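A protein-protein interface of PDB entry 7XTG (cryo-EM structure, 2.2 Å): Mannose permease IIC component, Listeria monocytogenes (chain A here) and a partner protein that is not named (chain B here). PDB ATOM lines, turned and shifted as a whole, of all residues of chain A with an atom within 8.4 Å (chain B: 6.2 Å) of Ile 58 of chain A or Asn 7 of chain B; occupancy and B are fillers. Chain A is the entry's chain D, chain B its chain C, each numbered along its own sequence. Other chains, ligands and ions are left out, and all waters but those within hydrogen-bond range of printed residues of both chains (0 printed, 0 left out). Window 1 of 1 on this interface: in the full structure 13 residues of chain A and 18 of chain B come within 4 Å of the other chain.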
ATOM      1  N   PRO A  31      15.933 -10.436  34.685  1.00  0.00           N
ATOM      2  CA  PRO A  31      16.892 -10.769  33.617  1.00  0.00           C
ATOM      3  C   PRO A  31      17.175  -9.621  32.661  1.00  0.00           C
ATOM      4  O   PRO A  31      18.317  -9.464  32.215  1.00  0.00           O
ATOM      5  CB  PRO A  31      16.219 -11.954  32.911  1.00  0.00           C
ATOM      6  CG  PRO A  31      15.323 -12.554  33.956  1.00  0.00           C
ATOM      7  CD  PRO A  31      14.825 -11.403  34.765  1.00  0.00           C
ATOM      8  N   LEU A  51      20.263 -11.849  25.788  1.00  0.00           N
ATOM      9  CA  LEU A  51      20.064 -12.891  26.789  1.00  0.00           C
ATOM     10  C   LEU A  51      19.109 -12.417  27.873  1.00  0.00           C
ATOM     11  O   LEU A  51      18.210 -13.158  28.288  1.00  0.00           O
ATOM     12  CB  LEU A  51      21.402 -13.293  27.405  1.00  0.00           C
ATOM     13  CG  LEU A  51      21.317 -14.000  28.761  1.00  0.00           C
ATOM     14  CD1 LEU A  51      21.124 -15.503  28.599  1.00  0.00           C
ATOM     15  CD2 LEU A  51      22.534 -13.691  29.625  1.00  0.00           C
ATOM     16  N   GLY A  52      19.283 -11.177  28.331  1.00  0.00           N
ATOM     17  CA  GLY A  52      18.341 -10.609  29.280  1.00  0.00           C
ATOM     18  C   GLY A  52      16.928 -10.548  28.737  1.00  0.00           C
ATOM     19  O   GLY A  52      15.967 -10.835  29.453  1.00  0.00           O
ATOM     20  N   GLY A  53      16.782 -10.171  27.466  1.00  0.00           N
ATOM     21  CA  GLY A  53      15.473 -10.235  26.838  1.00  0.00           C
ATOM     22  C   GLY A  53      14.960 -11.656  26.702  1.00  0.00           C
ATOM     23  O   GLY A  53      13.771 -11.920  26.906  1.00  0.00           O
ATOM     24  N   THR A  54      15.843 -12.588  26.342  1.00  0.00           N
ATOM     25  CA  THR A  54      15.435 -13.982  26.217  1.00  0.00           C
ATOM     26  C   THR A  54      15.073 -14.575  27.572  1.00  0.00           C
ATOM     27  O   THR A  54      14.067 -15.282  27.698  1.00  0.00           O
ATOM     28  CB  THR A  54      16.549 -14.800  25.567  1.00  0.00           C
ATOM     29  OG1 THR A  54      17.327 -13.958  24.710  1.00  0.00           O
ATOM     30  CG2 THR A  54      15.964 -15.931  24.744  1.00  0.00           C
ATOM     31  N   LEU A  55      15.884 -14.304  28.597  1.00  0.00           N
ATOM     32  CA  LEU A  55      15.654 -14.919  29.901  1.00  0.00           C
ATOM     33  C   LEU A  55      14.452 -14.301  30.605  1.00  0.00           C
ATOM     34  O   LEU A  55      13.703 -15.001  31.295  1.00  0.00           O
ATOM     35  CB  LEU A  55      16.906 -14.789  30.763  1.00  0.00           C
ATOM     36  CG  LEU A  55      16.990 -15.684  31.997  1.00  0.00           C
ATOM     37  CD1 LEU A  55      16.537 -17.097  31.667  1.00  0.00           C
ATOM     38  CD2 LEU A  55      18.401 -15.687  32.561  1.00  0.00           C
ATOM     39  N   GLN A  56      14.251 -12.991  30.439  1.00  0.00           N
ATOM     40  CA  GLN A  56      13.092 -12.337  31.038  1.00  0.00           C
ATOM     41  C   GLN A  56      11.794 -12.985  30.579  1.00  0.00           C
ATOM     42  O   GLN A  56      10.832 -13.070  31.349  1.00  0.00           O
ATOM     43  CB  GLN A  56      13.105 -10.846  30.694  1.00  0.00           C
ATOM     44  CG  GLN A  56      11.844 -10.088  31.062  1.00  0.00           C
ATOM     45  CD  GLN A  56      12.048  -9.175  32.255  1.00  0.00           C
ATOM     46  OE1 GLN A  56      12.899  -9.431  33.106  1.00  0.00           O
ATOM     47  NE2 GLN A  56      11.276  -8.096  32.316  1.00  0.00           N
ATOM     48  N   MET A  57      11.766 -13.475  29.341  1.00  0.00           N
ATOM     49  CA  MET A  57      10.589 -14.180  28.856  1.00  0.00           C
ATOM     50  C   MET A  57      10.360 -15.478  29.622  1.00  0.00           C
ATOM     51  O   MET A  57       9.225 -15.786  30.000  1.00  0.00           O
ATOM     52  CB  MET A  57      10.731 -14.447  27.361  1.00  0.00           C
ATOM     53  CG  MET A  57       9.418 -14.788  26.702  1.00  0.00           C
ATOM     54  SD  MET A  57       8.692 -13.369  25.860  1.00  0.00           S
ATOM     55  CE  MET A  57       7.488 -12.818  27.064  1.00  0.00           C
ATOM     56  N   ILE A  58      11.422 -16.255  29.857  1.00  0.00           N
ATOM     57  CA  ILE A  58      11.262 -17.526  30.560  1.00  0.00           C
ATOM     58  C   ILE A  58      10.871 -17.283  32.013  1.00  0.00           C
ATOM     59  O   ILE A  58      10.066 -18.028  32.589  1.00  0.00           O
ATOM     60  CB  ILE A  58      12.543 -18.377  30.452  1.00  0.00           C
ATOM     61  CG1 ILE A  58      12.945 -18.571  28.991  1.00  0.00           C
ATOM     62  CG2 ILE A  58      12.331 -19.740  31.098  1.00  0.00           C
ATOM     63  CD1 ILE A  58      14.439 -18.756  28.791  1.00  0.00           C
ATOM     64  N   ALA A  59      11.422 -16.231  32.622  1.00  0.00           N
ATOM     65  CA  ALA A  59      11.203 -15.901  34.026  1.00  0.00           C
ATOM     66  C   ALA A  59      10.062 -14.912  34.223  1.00  0.00           C
ATOM     67  O   ALA A  59      10.069 -14.139  35.185  1.00  0.00           O
ATOM     68  CB  ALA A  59      12.486 -15.348  34.643  1.00  0.00           C
ATOM     69  N   LEU A  60       9.084 -14.922  33.320  1.00  0.00           N
ATOM     70  CA  LEU A  60       7.959 -14.004  33.426  1.00  0.00           C
ATOM     71  C   LEU A  60       7.117 -14.270  34.667  1.00  0.00           C
ATOM     72  O   LEU A  60       6.828 -13.339  35.428  1.00  0.00           O
ATOM     73  CB  LEU A  60       7.100 -14.122  32.172  1.00  0.00           C
ATOM     74  CG  LEU A  60       6.051 -13.057  31.882  1.00  0.00           C
ATOM     75  CD1 LEU A  60       6.600 -11.961  30.975  1.00  0.00           C
ATOM     76  CD2 LEU A  60       4.855 -13.746  31.261  1.00  0.00           C
ATOM     77  N   GLY A  61       6.743 -15.522  34.907  1.00  0.00           N
ATOM     78  CA  GLY A  61       5.795 -15.864  35.945  1.00  0.00           C
ATOM     79  C   GLY A  61       6.381 -16.255  37.281  1.00  0.00           C
ATOM     80  O   GLY A  61       5.653 -16.797  38.119  1.00  0.00           O
ATOM     81  N   TRP A  62       7.666 -16.000  37.516  1.00  0.00           N
ATOM     82  CA  TRP A  62       8.308 -16.384  38.773  1.00  0.00           C
ATOM     83  C   TRP A  62       8.121 -15.244  39.766  1.00  0.00           C
ATOM     84  O   TRP A  62       8.740 -14.184  39.641  1.00  0.00           O
ATOM     85  CB  TRP A  62       9.786 -16.715  38.567  1.00  0.00           C
ATOM     86  CG  TRP A  62      10.107 -17.609  37.378  1.00  0.00           C
ATOM     87  CD1 TRP A  62       9.221 -18.239  36.548  1.00  0.00           C
ATOM     88  CD2 TRP A  62      11.414 -17.980  36.916  1.00  0.00           C
ATOM     89  NE1 TRP A  62       9.894 -18.959  35.594  1.00  0.00           N
ATOM     90  CE2 TRP A  62      11.240 -18.823  35.802  1.00  0.00           C
ATOM     91  CE3 TRP A  62      12.714 -17.676  37.334  1.00  0.00           C
ATOM     92  CZ2 TRP A  62      12.311 -19.361  35.097  1.00  0.00           C
ATOM     93  CZ3 TRP A  62      13.780 -18.218  36.633  1.00  0.00           C
ATOM     94  CH2 TRP A  62      13.569 -19.051  35.529  1.00  0.00           C
ATOM     95  N   PRO A  71      11.870 -19.237  41.445  1.00  0.00           N
ATOM     96  CA  PRO A  71      13.159 -19.827  41.080  1.00  0.00           C
ATOM     97  C   PRO A  71      14.304 -18.838  40.921  1.00  0.00           C
ATOM     98  O   PRO A  71      15.014 -18.866  39.910  1.00  0.00           O
ATOM     99  CB  PRO A  71      12.837 -20.466  39.728  1.00  0.00           C
ATOM    100  CG  PRO A  71      11.410 -20.961  39.898  1.00  0.00           C
ATOM    101  CD  PRO A  71      10.797 -20.173  41.067  1.00  0.00           C
ATOM    102  N   ALA A  73      15.625 -15.763  40.208  1.00  0.00           N
ATOM    103  CA  ALA A  73      16.136 -15.228  38.952  1.00  0.00           C
ATOM    104  C   ALA A  73      17.384 -14.378  39.146  1.00  0.00           C
ATOM    105  O   ALA A  73      18.024 -14.006  38.157  1.00  0.00           O
ATOM    106  CB  ALA A  73      15.054 -14.412  38.251  1.00  0.00           C
ATOM    107  N   VAL A  94      24.428 -16.922  23.039  1.00  0.00           N
ATOM    108  CA  VAL A  94      23.170 -16.615  23.710  1.00  0.00           C
ATOM    109  C   VAL A  94      22.385 -17.898  23.953  1.00  0.00           C
ATOM    110  O   VAL A  94      21.788 -18.088  25.020  1.00  0.00           O
ATOM    111  CB  VAL A  94      22.365 -15.588  22.891  1.00  0.00           C
ATOM    112  CG1 VAL A  94      20.881 -15.755  23.139  1.00  0.00           C
ATOM    113  CG2 VAL A  94      22.791 -14.168  23.244  1.00  0.00           C
ATOM    114  N   ALA A  97      24.203 -20.289  26.926  1.00  0.00           N
ATOM    115  CA  ALA A  97      24.018 -19.886  28.316  1.00  0.00           C
ATOM    116  C   ALA A  97      22.574 -20.067  28.766  1.00  0.00           C
ATOM    117  O   ALA A  97      22.325 -20.504  29.894  1.00  0.00           O
ATOM    118  CB  ALA A  97      24.457 -18.434  28.504  1.00  0.00           C
ATOM    119  N   ILE A  98      21.613 -19.739  27.895  1.00  0.00           N
ATOM    120  CA  ILE A  98      20.199 -19.864  28.249  1.00  0.00           C
ATOM    121  C   ILE A  98      19.877 -21.289  28.684  1.00  0.00           C
ATOM    122  O   ILE A  98      19.080 -21.507  29.606  1.00  0.00           O
ATOM    123  CB  ILE A  98      19.314 -19.409  27.071  1.00  0.00           C
ATOM    124  CG1 ILE A  98      19.034 -17.908  27.143  1.00  0.00           C
ATOM    125  CG2 ILE A  98      18.003 -20.197  27.015  1.00  0.00           C
ATOM    126  CD1 ILE A  98      17.991 -17.540  28.181  1.00  0.00           C
ATOM    127  N   ALA A  99      20.503 -22.278  28.048  1.00  0.00           N
ATOM    128  CA  ALA A  99      20.252 -23.666  28.416  1.00  0.00           C
ATOM    129  C   ALA A  99      20.596 -23.946  29.876  1.00  0.00           C
ATOM    130  O   ALA A  99      19.930 -24.764  30.519  1.00  0.00           O
ATOM    131  CB  ALA A  99      21.041 -24.596  27.498  1.00  0.00           C
ATOM    132  N   ALA A 101      20.640 -21.575  32.334  1.00  0.00           N
ATOM    133  CA  ALA A 101      20.059 -20.606  33.259  1.00  0.00           C
ATOM    134  C   ALA A 101      19.033 -21.267  34.175  1.00  0.00           C
ATOM    135  O   ALA A 101      19.029 -21.032  35.389  1.00  0.00           O
ATOM    136  CB  ALA A 101      19.420 -19.454  32.483  1.00  0.00           C
ATOM    137  N   VAL A 102      18.153 -22.098  33.607  1.00  0.00           N
ATOM    138  CA  VAL A 102      17.089 -22.712  34.406  1.00  0.00           C
ATOM    139  C   VAL A 102      17.634 -23.633  35.492  1.00  0.00           C
ATOM    140  O   VAL A 102      17.194 -23.513  36.647  1.00  0.00           O
ATOM    141  CB  VAL A 102      16.077 -23.419  33.489  1.00  0.00           C
ATOM    142  CG1 VAL A 102      14.777 -23.675  34.239  1.00  0.00           C
ATOM    143  CG2 VAL A 102      15.830 -22.601  32.239  1.00  0.00           C
ATOM    144  N   ALA A 105      18.700 -21.425  37.935  1.00  0.00           N
ATOM    145  CA  ALA A 105      17.538 -20.869  38.624  1.00  0.00           C
ATOM    146  C   ALA A 105      17.073 -21.794  39.743  1.00  0.00           C
ATOM    147  O   ALA A 105      16.683 -21.329  40.821  1.00  0.00           O
ATOM    148  CB  ALA A 105      16.405 -20.616  37.629  1.00  0.00           C
ATOM    149  N   GLY A 187      12.397 -29.180  32.134  1.00  0.00           N
ATOM    150  CA  GLY A 187      11.927 -27.833  32.410  1.00  0.00           C
ATOM    151  C   GLY A 187      10.458 -27.636  32.094  1.00  0.00           C
ATOM    152  O   GLY A 187       9.772 -26.863  32.770  1.00  0.00           O
ATOM    153  N   VAL A 191       6.252 -27.221  35.936  1.00  0.00           N
ATOM    154  CA  VAL A 191       5.010 -26.510  36.229  1.00  0.00           C
ATOM    155  C   VAL A 191       3.925 -27.414  36.795  1.00  0.00           C
ATOM    156  O   VAL A 191       2.887 -26.915  37.243  1.00  0.00           O
ATOM    157  CB  VAL A 191       4.483 -25.800  34.966  1.00  0.00           C
ATOM    158  CG1 VAL A 191       5.306 -24.554  34.673  1.00  0.00           C
ATOM    159  CG2 VAL A 191       4.493 -26.753  33.773  1.00  0.00           C
ATOM    160  N   TYR B   5      11.018 -23.982  25.833  1.00  0.00           N
ATOM    161  CA  TYR B   5      11.330 -23.355  27.115  1.00  0.00           C
ATOM    162  C   TYR B   5      10.177 -22.528  27.666  1.00  0.00           C
ATOM    163  O   TYR B   5      10.353 -21.837  28.678  1.00  0.00           O
ATOM    164  CB  TYR B   5      12.577 -22.475  27.005  1.00  0.00           C
ATOM    165  CG  TYR B   5      13.839 -23.166  27.450  1.00  0.00           C
ATOM    166  CD1 TYR B   5      13.859 -24.535  27.663  1.00  0.00           C
ATOM    167  CD2 TYR B   5      15.013 -22.454  27.649  1.00  0.00           C
ATOM    168  CE1 TYR B   5      15.010 -25.178  28.074  1.00  0.00           C
ATOM    169  CE2 TYR B   5      16.170 -23.092  28.051  1.00  0.00           C
ATOM    170  CZ  TYR B   5      16.163 -24.451  28.261  1.00  0.00           C
ATOM    171  OH  TYR B   5      17.314 -25.083  28.662  1.00  0.00           O
ATOM    172  N   GLY B   6       9.019 -22.557  27.025  1.00  0.00           N
ATOM    173  CA  GLY B   6       7.858 -21.887  27.584  1.00  0.00           C
ATOM    174  C   GLY B   6       7.830 -20.404  27.277  1.00  0.00           C
ATOM    175  O   GLY B   6       8.820 -19.799  26.864  1.00  0.00           O
ATOM    176  N   ASN B   7       6.654 -19.808  27.489  1.00  0.00           N
ATOM    177  CA  ASN B   7       6.427 -18.373  27.306  1.00  0.00           C
ATOM    178  C   ASN B   7       6.708 -17.926  25.873  1.00  0.00           C
ATOM    179  O   ASN B   7       7.049 -16.768  25.629  1.00  0.00           O
ATOM    180  CB  ASN B   7       7.261 -17.554  28.295  1.00  0.00           C
ATOM    181  CG  ASN B   7       6.897 -17.843  29.740  1.00  0.00           C
ATOM    182  OD1 ASN B   7       7.764 -18.171  30.556  1.00  0.00           O
ATOM    183  ND2 ASN B   7       5.613 -17.731  30.066  1.00  0.00           N
ATOM    184  N   GLY B   8       6.578 -18.843  24.917  1.00  0.00           N
ATOM    185  CA  GLY B   8       6.746 -18.530  23.514  1.00  0.00           C
ATOM    186  C   GLY B   8       8.148 -18.679  22.959  1.00  0.00           C
ATOM    187  O   GLY B   8       8.319 -18.613  21.736  1.00  0.00           O
ATOM    188  N   VAL B   9       9.154 -18.873  23.805  1.00  0.00           N
ATOM    189  CA  VAL B   9      10.534 -19.012  23.346  1.00  0.00           C
ATOM    190  C   VAL B   9      10.960 -20.459  23.521  1.00  0.00           C
ATOM    191  O   VAL B   9      10.917 -20.995  24.633  1.00  0.00           O
ATOM    192  CB  VAL B   9      11.477 -18.061  24.100  1.00  0.00           C
ATOM    193  CG1 VAL B   9      11.060 -17.924  25.555  1.00  0.00           C
ATOM    194  CG2 VAL B   9      12.920 -18.553  23.994  1.00  0.00           C
ATOM    195  N   VAL B  18      11.208 -15.891  20.315  1.00  0.00           N
ATOM    196  CA  VAL B  18       9.965 -15.932  21.074  1.00  0.00           C
ATOM    197  C   VAL B  18       8.806 -15.927  20.091  1.00  0.00           C
ATOM    198  O   VAL B  18       8.792 -15.129  19.146  1.00  0.00           O
ATOM    199  CB  VAL B  18       9.844 -14.750  22.051  1.00  0.00           C
ATOM    200  CG1 VAL B  18       8.528 -14.841  22.799  1.00  0.00           C
ATOM    201  CG2 VAL B  18      11.017 -14.730  23.012  1.00  0.00           C
ATOM    202  N   ASN B  19       7.848 -16.830  20.302  1.00  0.00           N
ATOM    203  CA  ASN B  19       6.626 -16.880  19.505  1.00  0.00           C
ATOM    204  C   ASN B  19       5.586 -15.978  20.155  1.00  0.00           C
ATOM    205  O   ASN B  19       5.225 -16.176  21.320  1.00  0.00           O
ATOM    206  CB  ASN B  19       6.116 -18.314  19.403  1.00  0.00           C
ATOM    207  CG  ASN B  19       5.190 -18.521  18.220  1.00  0.00           C
ATOM    208  OD1 ASN B  19       3.987 -18.272  18.306  1.00  0.00           O
ATOM    209  ND2 ASN B  19       5.747 -18.989  17.110  1.00  0.00           N
ATOM    210  N   GLU B  22       2.267 -17.770  21.511  1.00  0.00           N
ATOM    211  CA  GLU B  22       2.436 -18.484  22.772  1.00  0.00           C
ATOM    212  C   GLU B  22       2.811 -17.537  23.903  1.00  0.00           C
ATOM    213  O   GLU B  22       2.521 -17.822  25.070  1.00  0.00           O
ATOM    214  CB  GLU B  22       3.494 -19.578  22.626  1.00  0.00           C
ATOM    215  CG  GLU B  22       2.936 -20.957  22.309  1.00  0.00           C
ATOM    216  CD  GLU B  22       2.924 -21.252  20.822  1.00  0.00           C
ATOM    217  OE1 GLU B  22       3.244 -22.395  20.431  1.00  0.00           O
ATOM    218  OE2 GLU B  22       2.597 -20.338  20.039  1.00  0.00           O
ATOM    219  N   ALA B  23       3.478 -16.425  23.589  1.00  0.00           N
ATOM    220  CA  ALA B  23       3.754 -15.421  24.611  1.00  0.00           C
ATOM    221  C   ALA B  23       2.473 -14.732  25.061  1.00  0.00           C
ATOM    222  O   ALA B  23       2.291 -14.466  26.254  1.00  0.00           O
ATOM    223  CB  ALA B  23       4.768 -14.403  24.090  1.00  0.00           C
ATOM    224  N   THR B  24       1.570 -14.446  24.120  1.00  0.00           N
ATOM    225  CA  THR B  24       0.311 -13.794  24.470  1.00  0.00           C
ATOM    226  C   THR B  24      -0.587 -14.702  25.300  1.00  0.00           C
ATOM    227  O   THR B  24      -1.293 -14.231  26.197  1.00  0.00           O
ATOM    228  CB  THR B  24      -0.421 -13.339  23.210  1.00  0.00           C
ATOM    229  OG1 THR B  24       0.512 -12.749  22.299  1.00  0.00           O
ATOM    230  CG2 THR B  24      -1.484 -12.314  23.569  1.00  0.00           C
ATOM    231  N   SER B  26       0.454 -17.144  27.313  1.00  0.00           N
ATOM    232  CA  SER B  26       1.049 -17.257  28.643  1.00  0.00           C
ATOM    233  C   SER B  26       0.863 -15.977  29.453  1.00  0.00           C
ATOM    234  O   SER B  26       0.700 -16.032  30.677  1.00  0.00           O
ATOM    235  CB  SER B  26       2.529 -17.619  28.533  1.00  0.00           C
ATOM    236  OG  SER B  26       2.695 -18.999  28.255  1.00  0.00           O
ATOM    237  N   ILE B  27       0.886 -14.816  28.794  1.00  0.00           N
ATOM    238  CA  ILE B  27       0.647 -13.560  29.504  1.00  0.00           C
ATOM    239  C   ILE B  27      -0.788 -13.506  30.018  1.00  0.00           C
ATOM    240  O   ILE B  27      -1.077 -12.848  31.023  1.00  0.00           O
ATOM    241  CB  ILE B  27       0.985 -12.356  28.599  1.00  0.00           C
ATOM    242  CG1 ILE B  27       1.429 -11.155  29.424  1.00  0.00           C
ATOM    243  CG2 ILE B  27      -0.203 -11.922  27.778  1.00  0.00           C
ATOM    244  CD1 ILE B  27       2.833 -11.247  29.885  1.00  0.00           C
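Among the printed residues, merely in contact across the chains: Met 57 of chain A with Val 9 of chain B (3.7 Å), Met 57 of chain A with Val 18 of chain B (3.4 Å), Ile 58 of chain A with Tyr 5 of chain B (3.8 Å), Ile 58 of chain A with Val 9 of chain B (3.97 Å), Leu 60 of chain A with Ile 27 of chain B (3.5 Å) and Ile 98 of chain A with Tyr 5 of chain B (3.6 Å).
Printed residues of chain B within 4 Å of Met 57 of chain A: Asn 7, Val 9 and Val 18. Trp 62 of chain A touches none of the printed residues of chain B. Printed residues of chain B within 4 Å of Ala 99 of chain A: Tyr 5. No residue of chain A comes within 4 Å of Gly 6 of chain B. Of chain A, only Met 57 (2.9 Å) and Ile 58 (3.1 Å) come within 4 Å of Asn 7 of chain B. Of the printed residues of chain A, Val 9 of chain B touches Met 57 and Ile 58. Of the printed residues of chain A, Val 18 of chain B touches Met 57 (3.4 Å). Printed residues of chain A within 4 Å of Ile 27 of chain B: Leu 60. The nearest residue of chain B that does not touch Ile 58 of chain A is Gly 6 of chain B (4.8 Å). The nearest printed residue of chain A that does not touch Val 18 of chain B is Thr 54 of chain A (5.4 Å).
The side-chain amide oxygen (OD1) of Asn 7 of chain B lies close to the backbone carbonyl oxygen (O) of Met 57 of chain A. OH of Tyr 5 of chain B sits at hydrogen-bond distance from O of Ala 99 of chain A. The side-chain amide oxygen (OD1) of Asn 7 of chain B sits close to the backbone carbonyl oxygen (O) of Ile 58 of chain A, 3.1 Å away.
The indole nitrogen of Trp 62 of chain A lies within hydrogen-bond range of the backbone carbonyl oxygen of Ile 58 of chain A.
Of the 12 printed residues of chain B, 5 touch a printed residue of chain A. Hydrophobic or aromatic side chains of chain B that line the printed part of chain A: Tyr 5, Val 9, Val 18 and Ile 27. Of the 24 printed residues of chain A, 5 touch a printed residue of chain B. Hydrophobic or aromatic side chains of chain A that line the printed part of chain B: Met 57, Ile 58, Leu 60, Ile 98 and Ala 99. Among the printed residues, 9 pairs touch across the chains. Among the printed residues, no Asp or Glu carboxylate lies within 4 Å of a Lys or Arg side-chain nitrogen of the other chain.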
